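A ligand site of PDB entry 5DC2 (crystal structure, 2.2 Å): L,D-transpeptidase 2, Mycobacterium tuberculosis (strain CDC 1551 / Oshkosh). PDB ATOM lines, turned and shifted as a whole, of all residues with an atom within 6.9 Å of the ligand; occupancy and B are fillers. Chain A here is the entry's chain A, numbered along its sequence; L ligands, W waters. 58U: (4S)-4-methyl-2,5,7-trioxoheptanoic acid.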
ATOM      1  N   SER A 224      -7.503  18.737   9.483  1.00  0.00           N
ATOM      2  CA  SER A 224      -6.670  19.885   9.809  1.00  0.00           C
ATOM      3  C   SER A 224      -5.450  19.343  10.500  1.00  0.00           C
ATOM      4  O   SER A 224      -5.558  18.727  11.561  1.00  0.00           O
ATOM      5  CB  SER A 224      -7.407  20.881  10.699  1.00  0.00           C
ATOM      6  OG  SER A 224      -6.593  22.004  10.995  1.00  0.00           O
ATOM      7  N   MET A 225      -4.283  19.548   9.900  1.00  0.00           N
ATOM      8  CA  MET A 225      -3.045  19.008  10.439  1.00  0.00           C
ATOM      9  C   MET A 225      -2.262  20.114  11.148  1.00  0.00           C
ATOM     10  O   MET A 225      -2.821  21.171  11.455  1.00  0.00           O
ATOM     11  CB  MET A 225      -2.228  18.353   9.319  1.00  0.00           C
ATOM     12  CG  MET A 225      -2.875  17.058   8.800  1.00  0.00           C
ATOM     13  SD  MET A 225      -1.997  16.084   7.544  1.00  0.00           S
ATOM     14  CE  MET A 225      -2.024  17.216   6.156  1.00  0.00           C
ATOM     15  N   GLY A 226      -0.982  19.870  11.450  1.00  0.00           N
ATOM     16  CA  GLY A 226      -0.207  20.833  12.223  1.00  0.00           C
ATOM     17  C   GLY A 226       0.006  22.160  11.509  1.00  0.00           C
ATOM     18  O   GLY A 226       0.394  22.193  10.333  1.00  0.00           O
ATOM     19  N   LYS A 227      -0.226  23.257  12.230  1.00  0.00           N
ATOM     20  CA  LYS A 227       0.045  24.596  11.733  1.00  0.00           C
ATOM     21  C   LYS A 227       1.526  24.722  11.431  1.00  0.00           C
ATOM     22  O   LYS A 227       2.339  23.966  11.963  1.00  0.00           O
ATOM     23  CB  LYS A 227      -0.398  25.662  12.732  1.00  0.00           C
ATOM     24  CG  LYS A 227       0.251  25.529  14.092  1.00  0.00           C
ATOM     25  CD  LYS A 227      -0.396  26.447  15.123  1.00  0.00           C
ATOM     26  CE  LYS A 227       0.361  26.458  16.453  1.00  0.00           C
ATOM     27  NZ  LYS A 227       0.482  25.095  17.060  1.00  0.00           N
ATOM     28  N   THR A 230       4.087  24.228  14.001  1.00  0.00           N
ATOM     29  CA  THR A 230       4.119  22.896  14.600  1.00  0.00           C
ATOM     30  C   THR A 230       3.552  21.872  13.607  1.00  0.00           C
ATOM     31  O   THR A 230       2.502  21.272  13.849  1.00  0.00           O
ATOM     32  CB  THR A 230       3.335  22.822  15.936  1.00  0.00           C
ATOM     33  OG1 THR A 230       1.954  23.169  15.716  1.00  0.00           O
ATOM     34  CG2 THR A 230       3.950  23.775  16.985  1.00  0.00           C
ATOM     35  N   THR A 232       2.845  18.728  10.821  1.00  0.00           N
ATOM     36  CA  THR A 232       2.817  17.269  10.861  1.00  0.00           C
ATOM     37  C   THR A 232       3.920  16.781   9.945  1.00  0.00           C
ATOM     38  O   THR A 232       3.974  17.178   8.782  1.00  0.00           O
ATOM     39  CB  THR A 232       1.449  16.716  10.422  1.00  0.00           C
ATOM     40  OG1 THR A 232       0.408  17.278  11.218  1.00  0.00           O
ATOM     41  CG2 THR A 232       1.420  15.180  10.559  1.00  0.00           C
ATOM     42  N   MET A 248      -4.563  13.898  26.052  1.00  0.00           N
ATOM     43  CA  MET A 248      -3.303  14.133  25.382  1.00  0.00           C
ATOM     44  C   MET A 248      -2.521  15.226  26.096  1.00  0.00           C
ATOM     45  O   MET A 248      -2.947  16.365  26.192  1.00  0.00           O
ATOM     46  CB  MET A 248      -3.541  14.491  23.930  1.00  0.00           C
ATOM     47  CG  MET A 248      -3.949  13.294  23.094  1.00  0.00           C
ATOM     48  SD  MET A 248      -3.975  13.724  21.372  1.00  0.00           S
ATOM     49  CE  MET A 248      -5.151  15.082  21.381  1.00  0.00           C
ATOM     50  N   TYR A 253       5.315  13.754  25.553  1.00  0.00           N
ATOM     51  CA  TYR A 253       6.129  13.694  24.347  1.00  0.00           C
ATOM     52  C   TYR A 253       7.197  14.776  24.318  1.00  0.00           C
ATOM     53  O   TYR A 253       7.663  15.157  23.248  1.00  0.00           O
ATOM     54  CB  TYR A 253       5.251  13.804  23.086  1.00  0.00           C
ATOM     55  CG  TYR A 253       3.981  12.992  23.210  1.00  0.00           C
ATOM     56  CD1 TYR A 253       4.018  11.604  23.144  1.00  0.00           C
ATOM     57  CD2 TYR A 253       2.757  13.615  23.411  1.00  0.00           C
ATOM     58  CE1 TYR A 253       2.864  10.861  23.282  1.00  0.00           C
ATOM     59  CE2 TYR A 253       1.603  12.872  23.549  1.00  0.00           C
ATOM     60  CZ  TYR A 253       1.667  11.499  23.486  1.00  0.00           C
ATOM     61  OH  TYR A 253       0.523  10.760  23.615  1.00  0.00           O
ATOM     62  N   TYR A 263       0.395  21.616  25.539  1.00  0.00           N
ATOM     63  CA  TYR A 263      -1.043  21.434  25.597  1.00  0.00           C
ATOM     64  C   TYR A 263      -1.382  20.298  26.543  1.00  0.00           C
ATOM     65  O   TYR A 263      -0.544  19.421  26.815  1.00  0.00           O
ATOM     66  CB  TYR A 263      -1.601  21.145  24.207  1.00  0.00           C
ATOM     67  CG  TYR A 263      -0.941  19.959  23.568  1.00  0.00           C
ATOM     68  CD1 TYR A 263      -1.343  18.666  23.876  1.00  0.00           C
ATOM     69  CD2 TYR A 263       0.116  20.127  22.684  1.00  0.00           C
ATOM     70  CE1 TYR A 263      -0.722  17.564  23.315  1.00  0.00           C
ATOM     71  CE2 TYR A 263       0.747  19.041  22.109  1.00  0.00           C
ATOM     72  CZ  TYR A 263       0.320  17.761  22.426  1.00  0.00           C
ATOM     73  OH  TYR A 263       0.928  16.670  21.855  1.00  0.00           O
ATOM     74  N   THR A 265      -5.068  18.216  26.663  1.00  0.00           N
ATOM     75  CA  THR A 265      -6.411  18.214  26.085  1.00  0.00           C
ATOM     76  C   THR A 265      -7.086  16.853  26.168  1.00  0.00           C
ATOM     77  O   THR A 265      -6.509  15.830  25.774  1.00  0.00           O
ATOM     78  CB  THR A 265      -6.395  18.616  24.591  1.00  0.00           C
ATOM     79  OG1 THR A 265      -5.745  19.886  24.445  1.00  0.00           O
ATOM     80  CG2 THR A 265      -7.808  18.683  24.029  1.00  0.00           C
ATOM     81  N   VAL A 267      -9.589  14.353  24.548  1.00  0.00           N
ATOM     82  CA  VAL A 267     -10.147  14.149  23.205  1.00  0.00           C
ATOM     83  C   VAL A 267     -10.814  12.783  23.077  1.00  0.00           C
ATOM     84  O   VAL A 267     -10.495  11.849  23.812  1.00  0.00           O
ATOM     85  CB  VAL A 267      -9.068  14.257  22.104  1.00  0.00           C
ATOM     86  CG1 VAL A 267      -8.280  15.536  22.273  1.00  0.00           C
ATOM     87  CG2 VAL A 267      -8.133  13.036  22.115  1.00  0.00           C
ATOM     88  N   SER A 276       5.918  10.025  18.960  1.00  0.00           N
ATOM     89  CA  SER A 276       6.125  11.462  19.136  1.00  0.00           C
ATOM     90  C   SER A 276       4.833  12.186  19.477  1.00  0.00           C
ATOM     91  O   SER A 276       4.832  13.383  19.743  1.00  0.00           O
ATOM     92  CB  SER A 276       6.750  12.069  17.875  1.00  0.00           C
ATOM     93  OG  SER A 276       5.829  12.022  16.796  1.00  0.00           O
ATOM     94  N   GLY A 277       3.711  11.459  19.462  1.00  0.00           N
ATOM     95  CA  GLY A 277       2.451  11.992  19.922  1.00  0.00           C
ATOM     96  C   GLY A 277       1.429  12.391  18.871  1.00  0.00           C
ATOM     97  O   GLY A 277       0.435  13.048  19.183  1.00  0.00           O
ATOM     98  N   VAL A 278       1.650  12.011  17.629  1.00  0.00           N
ATOM     99  CA  VAL A 278       0.642  12.217  16.590  1.00  0.00           C
ATOM    100  C   VAL A 278      -0.502  11.201  16.725  1.00  0.00           C
ATOM    101  O   VAL A 278      -0.269   9.994  16.814  1.00  0.00           O
ATOM    102  CB  VAL A 278       1.267  12.163  15.181  1.00  0.00           C
ATOM    103  CG1 VAL A 278       0.202  12.405  14.074  1.00  0.00           C
ATOM    104  CG2 VAL A 278       2.424  13.180  15.050  1.00  0.00           C
ATOM    105  N   PHE A 279      -1.726  11.718  16.787  1.00  0.00           N
ATOM    106  CA  PHE A 279      -2.951  10.922  16.717  1.00  0.00           C
ATOM    107  C   PHE A 279      -3.866  11.423  15.606  1.00  0.00           C
ATOM    108  O   PHE A 279      -3.830  12.605  15.236  1.00  0.00           O
ATOM    109  CB  PHE A 279      -3.777  10.984  18.008  1.00  0.00           C
ATOM    110  CG  PHE A 279      -3.102  10.385  19.221  1.00  0.00           C
ATOM    111  CD1 PHE A 279      -2.038  11.019  19.827  1.00  0.00           C
ATOM    112  CD2 PHE A 279      -3.617   9.232  19.808  1.00  0.00           C
ATOM    113  CE1 PHE A 279      -1.464  10.487  20.967  1.00  0.00           C
ATOM    114  CE2 PHE A 279      -3.060   8.702  20.952  1.00  0.00           C
ATOM    115  CZ  PHE A 279      -1.980   9.320  21.537  1.00  0.00           C
ATOM    116  N   HIS A 281      -7.720  12.072  15.674  1.00  0.00           N
ATOM    117  CA  HIS A 281      -8.719  12.163  16.748  1.00  0.00           C
ATOM    118  C   HIS A 281      -9.833  13.152  16.449  1.00  0.00           C
ATOM    119  O   HIS A 281      -9.707  14.011  15.571  1.00  0.00           O
ATOM    120  CB  HIS A 281      -8.044  12.545  18.073  1.00  0.00           C
ATOM    121  CG  HIS A 281      -7.569  13.968  18.134  1.00  0.00           C
ATOM    122  ND1 HIS A 281      -8.433  15.036  18.343  1.00  0.00           N
ATOM    123  CD2 HIS A 281      -6.330  14.504  18.017  1.00  0.00           C
ATOM    124  CE1 HIS A 281      -7.737  16.158  18.350  1.00  0.00           C
ATOM    125  NE2 HIS A 281      -6.466  15.867  18.148  1.00  0.00           N
ATOM    126  N   ALA A 283     -11.974  16.285  16.627  1.00  0.00           N
ATOM    127  CA  ALA A 283     -11.706  17.698  16.925  1.00  0.00           C
ATOM    128  C   ALA A 283     -12.874  18.564  16.475  1.00  0.00           C
ATOM    129  O   ALA A 283     -12.840  19.181  15.412  1.00  0.00           O
ATOM    130  CB  ALA A 283     -10.428  18.151  16.233  1.00  0.00           C
ATOM    131  N   TRP A 285     -13.896  21.390  17.579  1.00  0.00           N
ATOM    132  CA  TRP A 285     -13.538  22.812  17.588  1.00  0.00           C
ATOM    133  C   TRP A 285     -12.908  23.300  16.274  1.00  0.00           C
ATOM    134  O   TRP A 285     -12.897  24.498  16.002  1.00  0.00           O
ATOM    135  CB  TRP A 285     -12.586  23.111  18.738  1.00  0.00           C
ATOM    136  CG  TRP A 285     -11.261  22.395  18.597  1.00  0.00           C
ATOM    137  CD1 TRP A 285     -10.150  22.829  17.922  1.00  0.00           C
ATOM    138  CD2 TRP A 285     -10.927  21.116  19.144  1.00  0.00           C
ATOM    139  NE1 TRP A 285      -9.146  21.894  18.015  1.00  0.00           N
ATOM    140  CE2 TRP A 285      -9.586  20.830  18.762  1.00  0.00           C
ATOM    141  CE3 TRP A 285     -11.625  20.178  19.922  1.00  0.00           C
ATOM    142  CZ2 TRP A 285      -8.941  19.645  19.144  1.00  0.00           C
ATOM    143  CZ3 TRP A 285     -10.964  19.004  20.294  1.00  0.00           C
ATOM    144  CH2 TRP A 285      -9.638  18.746  19.907  1.00  0.00           C
ATOM    145  N   SER A 286     -12.371  22.389  15.473  1.00  0.00           N
ATOM    146  CA  SER A 286     -11.733  22.816  14.219  1.00  0.00           C
ATOM    147  C   SER A 286     -12.432  22.281  12.967  1.00  0.00           C
ATOM    148  O   SER A 286     -11.830  22.281  11.879  1.00  0.00           O
ATOM    149  CB  SER A 286     -10.265  22.372  14.191  1.00  0.00           C
ATOM    150  OG  SER A 286     -10.173  20.959  14.143  1.00  0.00           O
ATOM    151  N   THR A 295      -4.337  23.750  11.762  1.00  0.00           N
ATOM    152  CA  THR A 295      -4.444  24.493  13.014  1.00  0.00           C
ATOM    153  C   THR A 295      -3.967  23.740  14.263  1.00  0.00           C
ATOM    154  O   THR A 295      -4.064  24.271  15.376  1.00  0.00           O
ATOM    155  CB  THR A 295      -5.882  24.908  13.290  1.00  0.00           C
ATOM    156  OG1 THR A 295      -6.692  23.736  13.421  1.00  0.00           O
ATOM    157  CG2 THR A 295      -6.410  25.771  12.149  1.00  0.00           C
ATOM    158  N   SER A 296      -3.479  22.509  14.112  1.00  0.00           N
ATOM    159  CA  SER A 296      -3.178  21.714  15.293  1.00  0.00           C
ATOM    160  C   SER A 296      -1.718  21.800  15.665  1.00  0.00           C
ATOM    161  O   SER A 296      -0.947  22.509  15.024  1.00  0.00           O
ATOM    162  CB  SER A 296      -3.567  20.243  15.112  1.00  0.00           C
ATOM    163  OG  SER A 296      -2.695  19.548  14.230  1.00  0.00           O
ATOM    164  N   HIS A 297      -1.367  21.061  16.718  1.00  0.00           N
ATOM    165  CA  HIS A 297       0.001  20.880  17.195  1.00  0.00           C
ATOM    166  C   HIS A 297       0.690  19.729  16.451  1.00  0.00           C
ATOM    167  O   HIS A 297       1.860  19.420  16.695  1.00  0.00           O
ATOM    168  CB  HIS A 297       0.016  20.601  18.697  1.00  0.00           C
ATOM    169  CG  HIS A 297      -0.371  21.786  19.533  1.00  0.00           C
ATOM    170  ND1 HIS A 297      -1.676  22.114  19.810  1.00  0.00           N
ATOM    171  CD2 HIS A 297       0.391  22.725  20.142  1.00  0.00           C
ATOM    172  CE1 HIS A 297      -1.713  23.207  20.555  1.00  0.00           C
ATOM    173  NE2 HIS A 297      -0.478  23.598  20.774  1.00  0.00           N
ATOM    174  N   GLY A 298      -0.035  19.071  15.554  1.00  0.00           N
ATOM    175  CA  GLY A 298       0.602  18.063  14.724  1.00  0.00           C
ATOM    176  C   GLY A 298      -0.304  16.891  14.449  1.00  0.00           C
ATOM    177  O   GLY A 298      -0.096  16.150  13.468  1.00  0.00           O
ATOM    178  N   CYS A 299      -1.312  16.715  15.296  1.00  0.00           N
ATOM    179  CA  CYS A 299      -2.292  15.649  15.113  1.00  0.00           C
ATOM    180  C   CYS A 299      -3.104  15.846  13.829  1.00  0.00           C
ATOM    181  O   CYS A 299      -3.168  16.948  13.276  1.00  0.00           O
ATOM    182  CB  CYS A 299      -3.256  15.559  16.291  1.00  0.00           C
ATOM    183  SG  CYS A 299      -2.510  15.009  17.859  1.00  0.00           S
ATOM    184  N   LEU A 300      -3.729  14.769  13.390  1.00  0.00           N
ATOM    185  CA  LEU A 300      -4.704  14.816  12.311  1.00  0.00           C
ATOM    186  C   LEU A 300      -6.077  15.035  12.934  1.00  0.00           C
ATOM    187  O   LEU A 300      -6.730  14.079  13.407  1.00  0.00           O
ATOM    188  CB  LEU A 300      -4.651  13.536  11.453  1.00  0.00           C
ATOM    189  CG  LEU A 300      -3.465  13.449  10.466  1.00  0.00           C
ATOM    190  CD1 LEU A 300      -2.113  13.655  11.125  1.00  0.00           C
ATOM    191  CD2 LEU A 300      -3.445  12.149   9.693  1.00  0.00           C
ATOM    192  N   ASN A 301      -6.492  16.302  13.006  1.00  0.00           N
ATOM    193  CA  ASN A 301      -7.847  16.658  13.412  1.00  0.00           C
ATOM    194  C   ASN A 301      -8.852  16.261  12.339  1.00  0.00           C
ATOM    195  O   ASN A 301      -8.711  16.645  11.166  1.00  0.00           O
ATOM    196  CB  ASN A 301      -7.970  18.168  13.672  1.00  0.00           C
ATOM    197  CG  ASN A 301      -7.254  18.617  14.918  1.00  0.00           C
ATOM    198  OD1 ASN A 301      -6.452  17.890  15.503  1.00  0.00           O
ATOM    199  ND2 ASN A 301      -7.532  19.853  15.321  1.00  0.00           N
HETATM  200  O12 58U L   1      -4.949  22.632  19.341  1.00  0.00           O
HETATM  201  C11 58U L   1      -5.233  21.694  18.559  1.00  0.00           C
HETATM  202  O13 58U L   1      -6.158  21.818  17.728  1.00  0.00           O
HETATM  203  C3  58U L   1      -4.478  20.455  18.628  1.00  0.00           C
HETATM  204  O4  58U L   1      -2.141  18.508  17.141  1.00  0.00           O
HETATM  205  C5  58U L   1      -2.712  18.028  18.123  1.00  0.00           C
HETATM  206  C6  58U L   1      -1.899  17.460  19.269  1.00  0.00           C
HETATM  207  C7  58U L   1      -1.454  16.077  18.869  1.00  0.00           C
HETATM  208  O14 58U L   1      -0.338  15.715  19.228  1.00  0.00           O
HETATM  209  C2  58U L   1      -4.973  19.234  17.838  1.00  0.00           C
HETATM  210  C1  58U L   1      -4.244  17.956  18.240  1.00  0.00           C
HETATM  211  C10 58U L   1      -4.599  17.641  19.695  1.00  0.00           C
HETATM  212  O16 58U L   1      -3.469  20.409  19.289  1.00  0.00           O
HETATM  213  O   HOH W   1      -0.567  14.387  21.393  1.00  0.00           O
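ND2 of Asn 301 is in hydrogen-bond range of O13 of the ligand. N of His 297 sits at hydrogen-bond distance from O4 of the ligand, 2.7 Å away. The backbone NH (N) of Cys 299 lies within hydrogen-bond range of an oxygen (O4) of the ligand, 2.7 Å away. The side-chain hydroxyl (OH) of Tyr 263 lies within hydrogen-bond range of an oxygen (O14) of the ligand, 3.1 Å away. SG of Cys 299 is bonded to C7 of the ligand (1.8 Å). The indole nitrogen of Trp 285 is in hydrogen-bond range of an oxygen (O13) of the ligand (3.0 Å). An oxygen (O16) of the ligand sits at hydrogen-bond distance from a ring nitrogen (ND1) of His 297 (2.5 Å). N of Gly 298 is in hydrogen-bond range of O4 of the ligand (2.7 Å). OG of Ser 296 sits close to O4 of the ligand, at 3.1 Å.
The side-chain sulfur of Cys 299 is in hydrogen-bond range of the backbone NH of Phe 279 (3.5 Å). The backbone carbonyl oxygen (O) of Cys 299 sits at hydrogen-bond distance from the side-chain hydroxyl (OG) of Ser 296 (2.8 Å). O of Asn 301 sits at hydrogen-bond distance from N of Ser 224 (2.9 Å). N of Met 248 sits at hydrogen-bond distance from O of Thr 265 (2.8 Å). The backbone carbonyl oxygen (O) of Gly 298 lies within hydrogen-bond range of the side-chain hydroxyl (OG1) of Thr 232 (2.6 Å). The side-chain amide nitrogen (ND2) of Asn 301 lies within hydrogen-bond range of the side-chain hydroxyl (OG) of Ser 286 (3.1 Å). A ring nitrogen (NE2) of His 281 is in hydrogen-bond range of the side-chain amide oxygen (OD1) of Asn 301. The backbone NH of Gly 298 sits at hydrogen-bond distance from the side-chain hydroxyl of Ser 296 (3.0 Å).
O of Gly 277 lies close to O14 of the ligand. Merely in contact with the ligand: His 281 (3.0 Å), Met 248 (3.1 Å) and Thr 295 (3.99 Å). Hydrophobic or aromatic side chains that line the ligand: Met 248, Tyr 263, His 281, Trp 285 and His 297. Of the 26 residues printed, 11 come within 4 Å of the ligand. The nearest printed residue that does not touch the ligand is Val 278 (4.5 Å).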
